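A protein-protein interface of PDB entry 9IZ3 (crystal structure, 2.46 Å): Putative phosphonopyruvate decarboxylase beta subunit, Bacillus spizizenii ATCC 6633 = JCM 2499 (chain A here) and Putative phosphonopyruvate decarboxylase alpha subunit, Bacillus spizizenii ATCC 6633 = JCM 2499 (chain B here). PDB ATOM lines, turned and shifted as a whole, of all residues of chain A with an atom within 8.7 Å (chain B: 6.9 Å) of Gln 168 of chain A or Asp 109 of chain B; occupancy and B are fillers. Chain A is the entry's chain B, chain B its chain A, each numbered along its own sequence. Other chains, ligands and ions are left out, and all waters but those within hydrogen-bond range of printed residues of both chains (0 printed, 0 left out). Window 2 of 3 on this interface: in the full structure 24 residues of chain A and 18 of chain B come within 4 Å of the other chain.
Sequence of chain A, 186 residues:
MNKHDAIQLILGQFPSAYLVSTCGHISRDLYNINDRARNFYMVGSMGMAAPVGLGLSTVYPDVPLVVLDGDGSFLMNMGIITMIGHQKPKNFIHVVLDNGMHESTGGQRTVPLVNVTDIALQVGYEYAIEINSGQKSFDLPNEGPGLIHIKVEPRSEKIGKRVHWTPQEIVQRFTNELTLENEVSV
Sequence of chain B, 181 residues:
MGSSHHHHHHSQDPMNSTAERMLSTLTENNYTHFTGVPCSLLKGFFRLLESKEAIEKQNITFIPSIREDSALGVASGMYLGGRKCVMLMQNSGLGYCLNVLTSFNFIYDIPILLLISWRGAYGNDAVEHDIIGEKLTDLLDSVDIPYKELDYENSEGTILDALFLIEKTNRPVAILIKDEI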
ATOM      1  N   PHE A  40      15.919  16.477 -15.969  1.00  0.00           N
ATOM      2  CA  PHE A  40      15.715  17.851 -15.525  1.00  0.00           C
ATOM      3  C   PHE A  40      15.546  17.840 -14.008  1.00  0.00           C
ATOM      4  O   PHE A  40      14.495  17.440 -13.493  1.00  0.00           O
ATOM      5  CB  PHE A  40      14.508  18.485 -16.215  1.00  0.00           C
ATOM      6  CG  PHE A  40      14.392  19.965 -15.982  1.00  0.00           C
ATOM      7  CD1 PHE A  40      13.767  20.458 -14.844  1.00  0.00           C
ATOM      8  CD2 PHE A  40      14.924  20.863 -16.891  1.00  0.00           C
ATOM      9  CE1 PHE A  40      13.669  21.818 -14.626  1.00  0.00           C
ATOM     10  CE2 PHE A  40      14.833  22.228 -16.678  1.00  0.00           C
ATOM     11  CZ  PHE A  40      14.203  22.710 -15.546  1.00  0.00           C
ATOM     12  N   TYR A  41      16.586  18.276 -13.298  1.00  0.00           N
ATOM     13  CA  TYR A  41      16.583  18.298 -11.841  1.00  0.00           C
ATOM     14  C   TYR A  41      15.976  19.591 -11.320  1.00  0.00           C
ATOM     15  O   TYR A  41      16.203  20.669 -11.879  1.00  0.00           O
ATOM     16  CB  TYR A  41      18.004  18.146 -11.297  1.00  0.00           C
ATOM     17  CG  TYR A  41      18.782  17.014 -11.925  1.00  0.00           C
ATOM     18  CD1 TYR A  41      18.547  15.700 -11.549  1.00  0.00           C
ATOM     19  CD2 TYR A  41      19.754  17.258 -12.891  1.00  0.00           C
ATOM     20  CE1 TYR A  41      19.250  14.660 -12.116  1.00  0.00           C
ATOM     21  CE2 TYR A  41      20.464  16.221 -13.466  1.00  0.00           C
ATOM     22  CZ  TYR A  41      20.206  14.922 -13.072  1.00  0.00           C
ATOM     23  OH  TYR A  41      20.896  13.870 -13.628  1.00  0.00           O
ATOM     24  N   VAL A  43      15.978  22.156  -8.171  1.00  0.00           N
ATOM     25  CA  VAL A  43      16.759  22.503  -6.989  1.00  0.00           C
ATOM     26  C   VAL A  43      15.840  22.872  -5.834  1.00  0.00           C
ATOM     27  O   VAL A  43      16.197  22.683  -4.665  1.00  0.00           O
ATOM     28  CB  VAL A  43      17.753  23.632  -7.305  1.00  0.00           C
ATOM     29  CG1 VAL A  43      18.784  23.149  -8.312  1.00  0.00           C
ATOM     30  CG2 VAL A  43      17.022  24.861  -7.827  1.00  0.00           C
ATOM     31  N   TRP A 165      25.738  20.568 -11.429  1.00  0.00           N
ATOM     32  CA  TRP A 165      25.397  21.265 -12.661  1.00  0.00           C
ATOM     33  C   TRP A 165      24.633  22.515 -12.264  1.00  0.00           C
ATOM     34  O   TRP A 165      23.701  22.439 -11.458  1.00  0.00           O
ATOM     35  CB  TRP A 165      24.540  20.408 -13.604  1.00  0.00           C
ATOM     36  CG  TRP A 165      25.222  19.192 -14.163  1.00  0.00           C
ATOM     37  CD1 TRP A 165      25.231  17.941 -13.622  1.00  0.00           C
ATOM     38  CD2 TRP A 165      25.975  19.106 -15.382  1.00  0.00           C
ATOM     39  NE1 TRP A 165      25.948  17.083 -14.419  1.00  0.00           N
ATOM     40  CE2 TRP A 165      26.416  17.773 -15.507  1.00  0.00           C
ATOM     41  CE3 TRP A 165      26.323  20.027 -16.375  1.00  0.00           C
ATOM     42  CZ2 TRP A 165      27.188  17.337 -16.584  1.00  0.00           C
ATOM     43  CZ3 TRP A 165      27.090  19.592 -17.445  1.00  0.00           C
ATOM     44  CH2 TRP A 165      27.512  18.259 -17.539  1.00  0.00           C
ATOM     45  N   THR A 166      25.028  23.662 -12.803  1.00  0.00           N
ATOM     46  CA  THR A 166      24.259  24.857 -12.524  1.00  0.00           C
ATOM     47  C   THR A 166      22.895  24.746 -13.209  1.00  0.00           C
ATOM     48  O   THR A 166      22.765  24.091 -14.246  1.00  0.00           O
ATOM     49  CB  THR A 166      25.003  26.115 -12.981  1.00  0.00           C
ATOM     50  OG1 THR A 166      24.433  27.269 -12.351  1.00  0.00           O
ATOM     51  CG2 THR A 166      24.918  26.291 -14.477  1.00  0.00           C
ATOM     52  N   PRO A 167      21.853  25.316 -12.604  1.00  0.00           N
ATOM     53  CA  PRO A 167      20.516  25.259 -13.224  1.00  0.00           C
ATOM     54  C   PRO A 167      20.485  25.674 -14.689  1.00  0.00           C
ATOM     55  O   PRO A 167      19.753  25.063 -15.480  1.00  0.00           O
ATOM     56  CB  PRO A 167      19.700  26.208 -12.339  1.00  0.00           C
ATOM     57  CG  PRO A 167      20.333  26.068 -10.984  1.00  0.00           C
ATOM     58  CD  PRO A 167      21.799  25.781 -11.206  1.00  0.00           C
ATOM     59  N   GLN A 168      21.265  26.687 -15.078  1.00  0.00           N
ATOM     60  CA  GLN A 168      21.290  27.100 -16.478  1.00  0.00           C
ATOM     61  C   GLN A 168      21.867  26.002 -17.367  1.00  0.00           C
ATOM     62  O   GLN A 168      21.368  25.759 -18.476  1.00  0.00           O
ATOM     63  CB  GLN A 168      22.084  28.398 -16.627  1.00  0.00           C
ATOM     64  CG  GLN A 168      21.422  29.613 -15.982  1.00  0.00           C
ATOM     65  CD  GLN A 168      22.413  30.712 -15.637  1.00  0.00           C
ATOM     66  OE1 GLN A 168      23.429  30.888 -16.314  1.00  0.00           O
ATOM     67  NE2 GLN A 168      22.122  31.460 -14.576  1.00  0.00           N
ATOM     68  N   GLU A 169      22.913  25.318 -16.893  1.00  0.00           N
ATOM     69  CA  GLU A 169      23.463  24.197 -17.649  1.00  0.00           C
ATOM     70  C   GLU A 169      22.450  23.064 -17.764  1.00  0.00           C
ATOM     71  O   GLU A 169      22.335  22.430 -18.821  1.00  0.00           O
ATOM     72  CB  GLU A 169      24.755  23.706 -16.996  1.00  0.00           C
ATOM     73  CG  GLU A 169      25.973  24.557 -17.342  1.00  0.00           C
ATOM     74  CD  GLU A 169      27.261  24.009 -16.761  1.00  0.00           C
ATOM     75  OE1 GLU A 169      28.224  23.805 -17.534  1.00  0.00           O
ATOM     76  OE2 GLU A 169      27.313  23.781 -15.533  1.00  0.00           O
ATOM     77  N   ILE A 170      21.717  22.788 -16.679  1.00  0.00           N
ATOM     78  CA  ILE A 170      20.639  21.801 -16.728  1.00  0.00           C
ATOM     79  C   ILE A 170      19.651  22.159 -17.829  1.00  0.00           C
ATOM     80  O   ILE A 170      19.303  21.325 -18.677  1.00  0.00           O
ATOM     81  CB  ILE A 170      19.937  21.708 -15.360  1.00  0.00           C
ATOM     82  CG1 ILE A 170      20.806  20.957 -14.351  1.00  0.00           C
ATOM     83  CG2 ILE A 170      18.566  21.048 -15.497  1.00  0.00           C
ATOM     84  CD1 ILE A 170      20.251  20.983 -12.937  1.00  0.00           C
ATOM     85  N   VAL A 171      19.197  23.416 -17.831  1.00  0.00           N
ATOM     86  CA  VAL A 171      18.243  23.879 -18.838  1.00  0.00           C
ATOM     87  C   VAL A 171      18.794  23.644 -20.235  1.00  0.00           C
ATOM     88  O   VAL A 171      18.115  23.083 -21.101  1.00  0.00           O
ATOM     89  CB  VAL A 171      17.902  25.364 -18.613  1.00  0.00           C
ATOM     90  CG1 VAL A 171      17.247  25.952 -19.857  1.00  0.00           C
ATOM     91  CG2 VAL A 171      16.997  25.528 -17.405  1.00  0.00           C
ATOM     92  N   GLN A 172      20.040  24.070 -20.471  1.00  0.00           N
ATOM     93  CA  GLN A 172      20.599  24.014 -21.820  1.00  0.00           C
ATOM     94  C   GLN A 172      20.745  22.575 -22.301  1.00  0.00           C
ATOM     95  O   GLN A 172      20.296  22.232 -23.402  1.00  0.00           O
ATOM     96  CB  GLN A 172      21.944  24.741 -21.864  1.00  0.00           C
ATOM     97  CG  GLN A 172      22.606  24.723 -23.233  1.00  0.00           C
ATOM     98  CD  GLN A 172      23.675  23.654 -23.342  1.00  0.00           C
ATOM     99  OE1 GLN A 172      24.563  23.560 -22.494  1.00  0.00           O
ATOM    100  NE2 GLN A 172      23.586  22.830 -24.382  1.00  0.00           N
ATOM    101  N   ARG A 173      21.375  21.718 -21.492  1.00  0.00           N
ATOM    102  CA  ARG A 173      21.501  20.307 -21.859  1.00  0.00           C
ATOM    103  C   ARG A 173      20.136  19.687 -22.147  1.00  0.00           C
ATOM    104  O   ARG A 173      19.942  19.029 -23.182  1.00  0.00           O
ATOM    105  CB  ARG A 173      22.209  19.536 -20.741  1.00  0.00           C
ATOM    106  CG  ARG A 173      23.603  20.037 -20.395  1.00  0.00           C
ATOM    107  CD  ARG A 173      24.478  18.906 -19.866  1.00  0.00           C
ATOM    108  NE  ARG A 173      23.801  18.126 -18.834  1.00  0.00           N
ATOM    109  CZ  ARG A 173      23.923  16.810 -18.688  1.00  0.00           C
ATOM    110  NH1 ARG A 173      23.267  16.184 -17.719  1.00  0.00           N
ATOM    111  NH2 ARG A 173      24.698  16.119 -19.512  1.00  0.00           N
ATOM    112  N   PHE A 174      19.169  19.902 -21.247  1.00  0.00           N
ATOM    113  CA  PHE A 174      17.874  19.236 -21.355  1.00  0.00           C
ATOM    114  C   PHE A 174      17.122  19.683 -22.604  1.00  0.00           C
ATOM    115  O   PHE A 174      16.636  18.853 -23.388  1.00  0.00           O
ATOM    116  CB  PHE A 174      17.058  19.514 -20.087  1.00  0.00           C
ATOM    117  CG  PHE A 174      15.728  18.821 -20.047  1.00  0.00           C
ATOM    118  CD1 PHE A 174      15.625  17.511 -19.610  1.00  0.00           C
ATOM    119  CD2 PHE A 174      14.575  19.487 -20.430  1.00  0.00           C
ATOM    120  CE1 PHE A 174      14.396  16.870 -19.566  1.00  0.00           C
ATOM    121  CE2 PHE A 174      13.342  18.855 -20.388  1.00  0.00           C
ATOM    122  CZ  PHE A 174      13.253  17.544 -19.955  1.00  0.00           C
ATOM    123  N   THR A 175      17.021  20.999 -22.814  1.00  0.00           N
ATOM    124  CA  THR A 175      16.279  21.480 -23.972  1.00  0.00           C
ATOM    125  C   THR A 175      17.013  21.173 -25.274  1.00  0.00           C
ATOM    126  O   THR A 175      16.363  20.939 -26.299  1.00  0.00           O
ATOM    127  CB  THR A 175      15.994  22.979 -23.855  1.00  0.00           C
ATOM    128  OG1 THR A 175      15.166  23.385 -24.952  1.00  0.00           O
ATOM    129  CG2 THR A 175      17.276  23.790 -23.893  1.00  0.00           C
ATOM    130  N   TYR B  79       7.792  26.298 -21.931  1.00  0.00           N
ATOM    131  CA  TYR B  79       8.994  26.992 -22.375  1.00  0.00           C
ATOM    132  C   TYR B  79      10.144  26.018 -22.582  1.00  0.00           C
ATOM    133  O   TYR B  79      10.889  26.124 -23.562  1.00  0.00           O
ATOM    134  CB  TYR B  79       9.393  28.073 -21.374  1.00  0.00           C
ATOM    135  CG  TYR B  79      10.676  28.767 -21.765  1.00  0.00           C
ATOM    136  CD1 TYR B  79      10.665  29.837 -22.649  1.00  0.00           C
ATOM    137  CD2 TYR B  79      11.903  28.336 -21.272  1.00  0.00           C
ATOM    138  CE1 TYR B  79      11.833  30.467 -23.020  1.00  0.00           C
ATOM    139  CE2 TYR B  79      13.075  28.960 -21.637  1.00  0.00           C
ATOM    140  CZ  TYR B  79      13.036  30.023 -22.512  1.00  0.00           C
ATOM    141  OH  TYR B  79      14.204  30.653 -22.878  1.00  0.00           O
ATOM    142  N   PHE B 104      12.859  29.254  -8.984  1.00  0.00           N
ATOM    143  CA  PHE B 104      12.885  28.441 -10.197  1.00  0.00           C
ATOM    144  C   PHE B 104      13.204  29.290 -11.421  1.00  0.00           C
ATOM    145  O   PHE B 104      14.303  29.171 -11.969  1.00  0.00           O
ATOM    146  CB  PHE B 104      11.552  27.704 -10.346  1.00  0.00           C
ATOM    147  CG  PHE B 104      11.499  26.789 -11.527  1.00  0.00           C
ATOM    148  CD1 PHE B 104      12.372  25.720 -11.624  1.00  0.00           C
ATOM    149  CD2 PHE B 104      10.581  26.998 -12.544  1.00  0.00           C
ATOM    150  CE1 PHE B 104      12.330  24.870 -12.711  1.00  0.00           C
ATOM    151  CE2 PHE B 104      10.533  26.150 -13.633  1.00  0.00           C
ATOM    152  CZ  PHE B 104      11.408  25.083 -13.717  1.00  0.00           C
ATOM    153  N   ASN B 105      12.285  30.151 -11.876  1.00  0.00           N
ATOM    154  CA  ASN B 105      12.495  30.859 -13.137  1.00  0.00           C
ATOM    155  C   ASN B 105      13.599  31.900 -13.059  1.00  0.00           C
ATOM    156  O   ASN B 105      14.222  32.197 -14.084  1.00  0.00           O
ATOM    157  CB  ASN B 105      11.201  31.525 -13.605  1.00  0.00           C
ATOM    158  CG  ASN B 105      10.006  30.600 -13.514  1.00  0.00           C
ATOM    159  OD1 ASN B 105       9.388  30.483 -12.458  1.00  0.00           O
ATOM    160  ND2 ASN B 105       9.672  29.941 -14.619  1.00  0.00           N
ATOM    161  N   PHE B 106      13.833  32.482 -11.887  1.00  0.00           N
ATOM    162  CA  PHE B 106      14.953  33.396 -11.733  1.00  0.00           C
ATOM    163  C   PHE B 106      16.249  32.669 -11.418  1.00  0.00           C
ATOM    164  O   PHE B 106      17.303  33.310 -11.339  1.00  0.00           O
ATOM    165  CB  PHE B 106      14.651  34.421 -10.645  1.00  0.00           C
ATOM    166  CG  PHE B 106      13.849  35.587 -11.128  1.00  0.00           C
ATOM    167  CD1 PHE B 106      13.092  35.500 -12.285  1.00  0.00           C
ATOM    168  CD2 PHE B 106      13.854  36.776 -10.431  1.00  0.00           C
ATOM    169  CE1 PHE B 106      12.360  36.580 -12.729  1.00  0.00           C
ATOM    170  CE2 PHE B 106      13.123  37.849 -10.873  1.00  0.00           C
ATOM    171  CZ  PHE B 106      12.374  37.752 -12.023  1.00  0.00           C
ATOM    172  N   ILE B 107      16.189  31.355 -11.240  1.00  0.00           N
ATOM    173  CA  ILE B 107      17.368  30.535 -11.023  1.00  0.00           C
ATOM    174  C   ILE B 107      17.728  29.741 -12.271  1.00  0.00           C
ATOM    175  O   ILE B 107      18.906  29.588 -12.598  1.00  0.00           O
ATOM    176  CB  ILE B 107      17.140  29.611  -9.803  1.00  0.00           C
ATOM    177  CG1 ILE B 107      17.659  30.264  -8.517  1.00  0.00           C
ATOM    178  CG2 ILE B 107      17.812  28.272  -9.991  1.00  0.00           C
ATOM    179  CD1 ILE B 107      17.044  31.602  -8.198  1.00  0.00           C
ATOM    180  N   TYR B 108      16.721  29.252 -12.993  1.00  0.00           N
ATOM    181  CA  TYR B 108      16.920  28.551 -14.256  1.00  0.00           C
ATOM    182  C   TYR B 108      16.862  29.479 -15.459  1.00  0.00           C
ATOM    183  O   TYR B 108      17.117  29.028 -16.580  1.00  0.00           O
ATOM    184  CB  TYR B 108      15.870  27.444 -14.420  1.00  0.00           C
ATOM    185  CG  TYR B 108      16.058  26.268 -13.489  1.00  0.00           C
ATOM    186  CD1 TYR B 108      15.677  26.345 -12.155  1.00  0.00           C
ATOM    187  CD2 TYR B 108      16.610  25.081 -13.944  1.00  0.00           C
ATOM    188  CE1 TYR B 108      15.845  25.271 -11.302  1.00  0.00           C
ATOM    189  CE2 TYR B 108      16.780  24.002 -13.099  1.00  0.00           C
ATOM    190  CZ  TYR B 108      16.398  24.102 -11.779  1.00  0.00           C
ATOM    191  OH  TYR B 108      16.572  23.024 -10.939  1.00  0.00           O
ATOM    192  N   ASP B 109      16.535  30.752 -15.252  1.00  0.00           N
ATOM    193  CA  ASP B 109      16.347  31.719 -16.331  1.00  0.00           C
ATOM    194  C   ASP B 109      15.325  31.204 -17.344  1.00  0.00           C
ATOM    195  O   ASP B 109      15.609  31.016 -18.526  1.00  0.00           O
ATOM    196  CB  ASP B 109      17.678  32.065 -17.002  1.00  0.00           C
ATOM    197  CG  ASP B 109      18.657  32.729 -16.048  1.00  0.00           C
ATOM    198  OD1 ASP B 109      18.206  33.450 -15.129  1.00  0.00           O
ATOM    199  OD2 ASP B 109      19.877  32.532 -16.218  1.00  0.00           O
ATOM    200  N   ILE B 110      14.115  30.967 -16.846  1.00  0.00           N
ATOM    201  CA  ILE B 110      13.003  30.549 -17.696  1.00  0.00           C
ATOM    202  C   ILE B 110      12.043  31.726 -17.826  1.00  0.00           C
ATOM    203  O   ILE B 110      11.247  31.983 -16.912  1.00  0.00           O
ATOM    204  CB  ILE B 110      12.306  29.301 -17.135  1.00  0.00           C
ATOM    205  CG1 ILE B 110      13.266  28.113 -17.152  1.00  0.00           C
ATOM    206  CG2 ILE B 110      11.058  28.969 -17.941  1.00  0.00           C
ATOM    207  CD1 ILE B 110      12.761  26.923 -16.375  1.00  0.00           C
ATOM    208  N   PRO B 111      12.094  32.474 -18.927  1.00  0.00           N
ATOM    209  CA  PRO B 111      11.255  33.673 -19.050  1.00  0.00           C
ATOM    210  C   PRO B 111       9.797  33.310 -19.296  1.00  0.00           C
ATOM    211  O   PRO B 111       9.473  32.520 -20.185  1.00  0.00           O
ATOM    212  CB  PRO B 111      11.855  34.405 -20.254  1.00  0.00           C
ATOM    213  CG  PRO B 111      12.493  33.327 -21.058  1.00  0.00           C
ATOM    214  CD  PRO B 111      13.005  32.316 -20.072  1.00  0.00           C
ATOM    215  N   THR B 169      16.948  39.505 -20.563  1.00  0.00           N
ATOM    216  CA  THR B 169      17.031  38.925 -19.235  1.00  0.00           C
ATOM    217  C   THR B 169      16.980  37.415 -19.264  1.00  0.00           C
ATOM    218  O   THR B 169      17.623  36.756 -18.437  1.00  0.00           O
ATOM    219  CB  THR B 169      15.851  39.425 -18.395  1.00  0.00           C
ATOM    220  OG1 THR B 169      15.549  40.773 -18.753  1.00  0.00           O
ATOM    221  CG2 THR B 169      16.152  39.329 -16.906  1.00  0.00           C
ATOM    222  N   ASN B 170      16.202  36.869 -20.196  1.00  0.00           N
ATOM    223  CA  ASN B 170      15.766  35.485 -20.135  1.00  0.00           C
ATOM    224  C   ASN B 170      15.150  35.185 -18.770  1.00  0.00           C
ATOM    225  O   ASN B 170      15.297  34.094 -18.221  1.00  0.00           O
ATOM    226  CB  ASN B 170      16.917  34.538 -20.459  1.00  0.00           C
ATOM    227  CG  ASN B 170      16.839  34.020 -21.872  1.00  0.00           C
ATOM    228  OD1 ASN B 170      16.264  34.670 -22.750  1.00  0.00           O
ATOM    229  ND2 ASN B 170      17.410  32.849 -22.107  1.00  0.00           N
ATOM    230  N   ARG B 171      14.452  36.173 -18.216  1.00  0.00           N
ATOM    231  CA  ARG B 171      13.735  36.049 -16.957  1.00  0.00           C
ATOM    232  C   ARG B 171      12.349  36.651 -17.124  1.00  0.00           C
ATOM    233  O   ARG B 171      12.144  37.518 -17.983  1.00  0.00           O
ATOM    234  CB  ARG B 171      14.471  36.764 -15.813  1.00  0.00           C
ATOM    235  CG  ARG B 171      15.501  35.926 -15.069  1.00  0.00           C
ATOM    236  CD  ARG B 171      16.605  36.828 -14.522  1.00  0.00           C
ATOM    237  NE  ARG B 171      17.575  36.095 -13.715  1.00  0.00           N
ATOM    238  CZ  ARG B 171      18.754  36.575 -13.326  1.00  0.00           C
ATOM    239  NH1 ARG B 171      19.136  37.799 -13.675  1.00  0.00           N
ATOM    240  NH2 ARG B 171      19.560  35.821 -12.592  1.00  0.00           N
ATOM    241  N   PRO B 172      11.375  36.210 -16.328  1.00  0.00           N
ATOM    242  CA  PRO B 172      10.025  36.777 -16.430  1.00  0.00           C
ATOM    243  C   PRO B 172       9.978  38.263 -16.084  1.00  0.00           C
ATOM    244  O   PRO B 172      10.631  38.730 -15.146  1.00  0.00           O
ATOM    245  CB  PRO B 172       9.206  35.943 -15.433  1.00  0.00           C
ATOM    246  CG  PRO B 172      10.168  35.043 -14.735  1.00  0.00           C
ATOM    247  CD  PRO B 172      11.391  34.945 -15.576  1.00  0.00           C
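N of Val 43 of chain A sits at hydrogen-bond distance from OH of Tyr 108 of chain B, at 3.0 Å. The side-chain carboxylate of Asp 109 of chain B is in hydrogen-bond range of the side-chain amide nitrogen of Gln 168 of chain A (3.0 Å). OH of Tyr 108 of chain B is in hydrogen-bond range of O of Tyr 41 of chain A, 2.6 Å away.
The side-chain carboxylate of Asp 109 of chain B is in salt-bridge range of the guanidinium group of Arg 171 of chain B.
Phe 40 of chain A touches Phe 104 of chain B (CE1 to CE1, 3.8 Å). CZ of Phe 40 of chain A touches CD2 of Tyr 108 of chain B, at 3.7 Å. CB of Pro 167 of chain A touches O of Ile 107 of chain B, at 3.5 Å. Pro 167 of chain A touches Tyr 108 of chain B (O to CD2, 3.5 Å). CG2 of Val 171 of chain A touches CD2 of Tyr 108 of chain B, 3.5 Å away.
Gln 168 of chain A touches just one residue of chain B: Asp 109. Of chain A, only Gln 168 (3.0 Å) comes within 4 Å of Asp 109 of chain B. Of the printed residues of chain A, Phe 104 of chain B touches Phe 40. Printed residues of chain A within 4 Å of Ile 107 of chain B: Pro 167 (3.5 Å). The nearest residue of chain B that does not touch Gln 168 of chain A is Ile 107 of chain B (4.2 Å). The nearest residue of chain A that does not touch Asp 109 of chain B is Val 171 of chain A (5.5 Å). The nearest printed residue of chain B that does not touch Phe 40 of chain A is Ile 110 of chain B (4.5 Å).
Of the 13 printed residues of chain B, 4 touch a printed residue of chain A. Printed residues of chain B that touch a printed residue of chain A: Phe 104, Ile 107, Tyr 108 and Asp 109. Hydrophobic or aromatic side chains of chain B that line the printed part of chain A: Phe 104, Ile 107 and Tyr 108. Of the 14 printed residues of chain A, 6 touch a printed residue of chain B. Hydrophobic or aromatic side chains of chain A within 4 Å of the printed part of chain B: Phe 40, Val 43, Pro 167 and Val 171.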
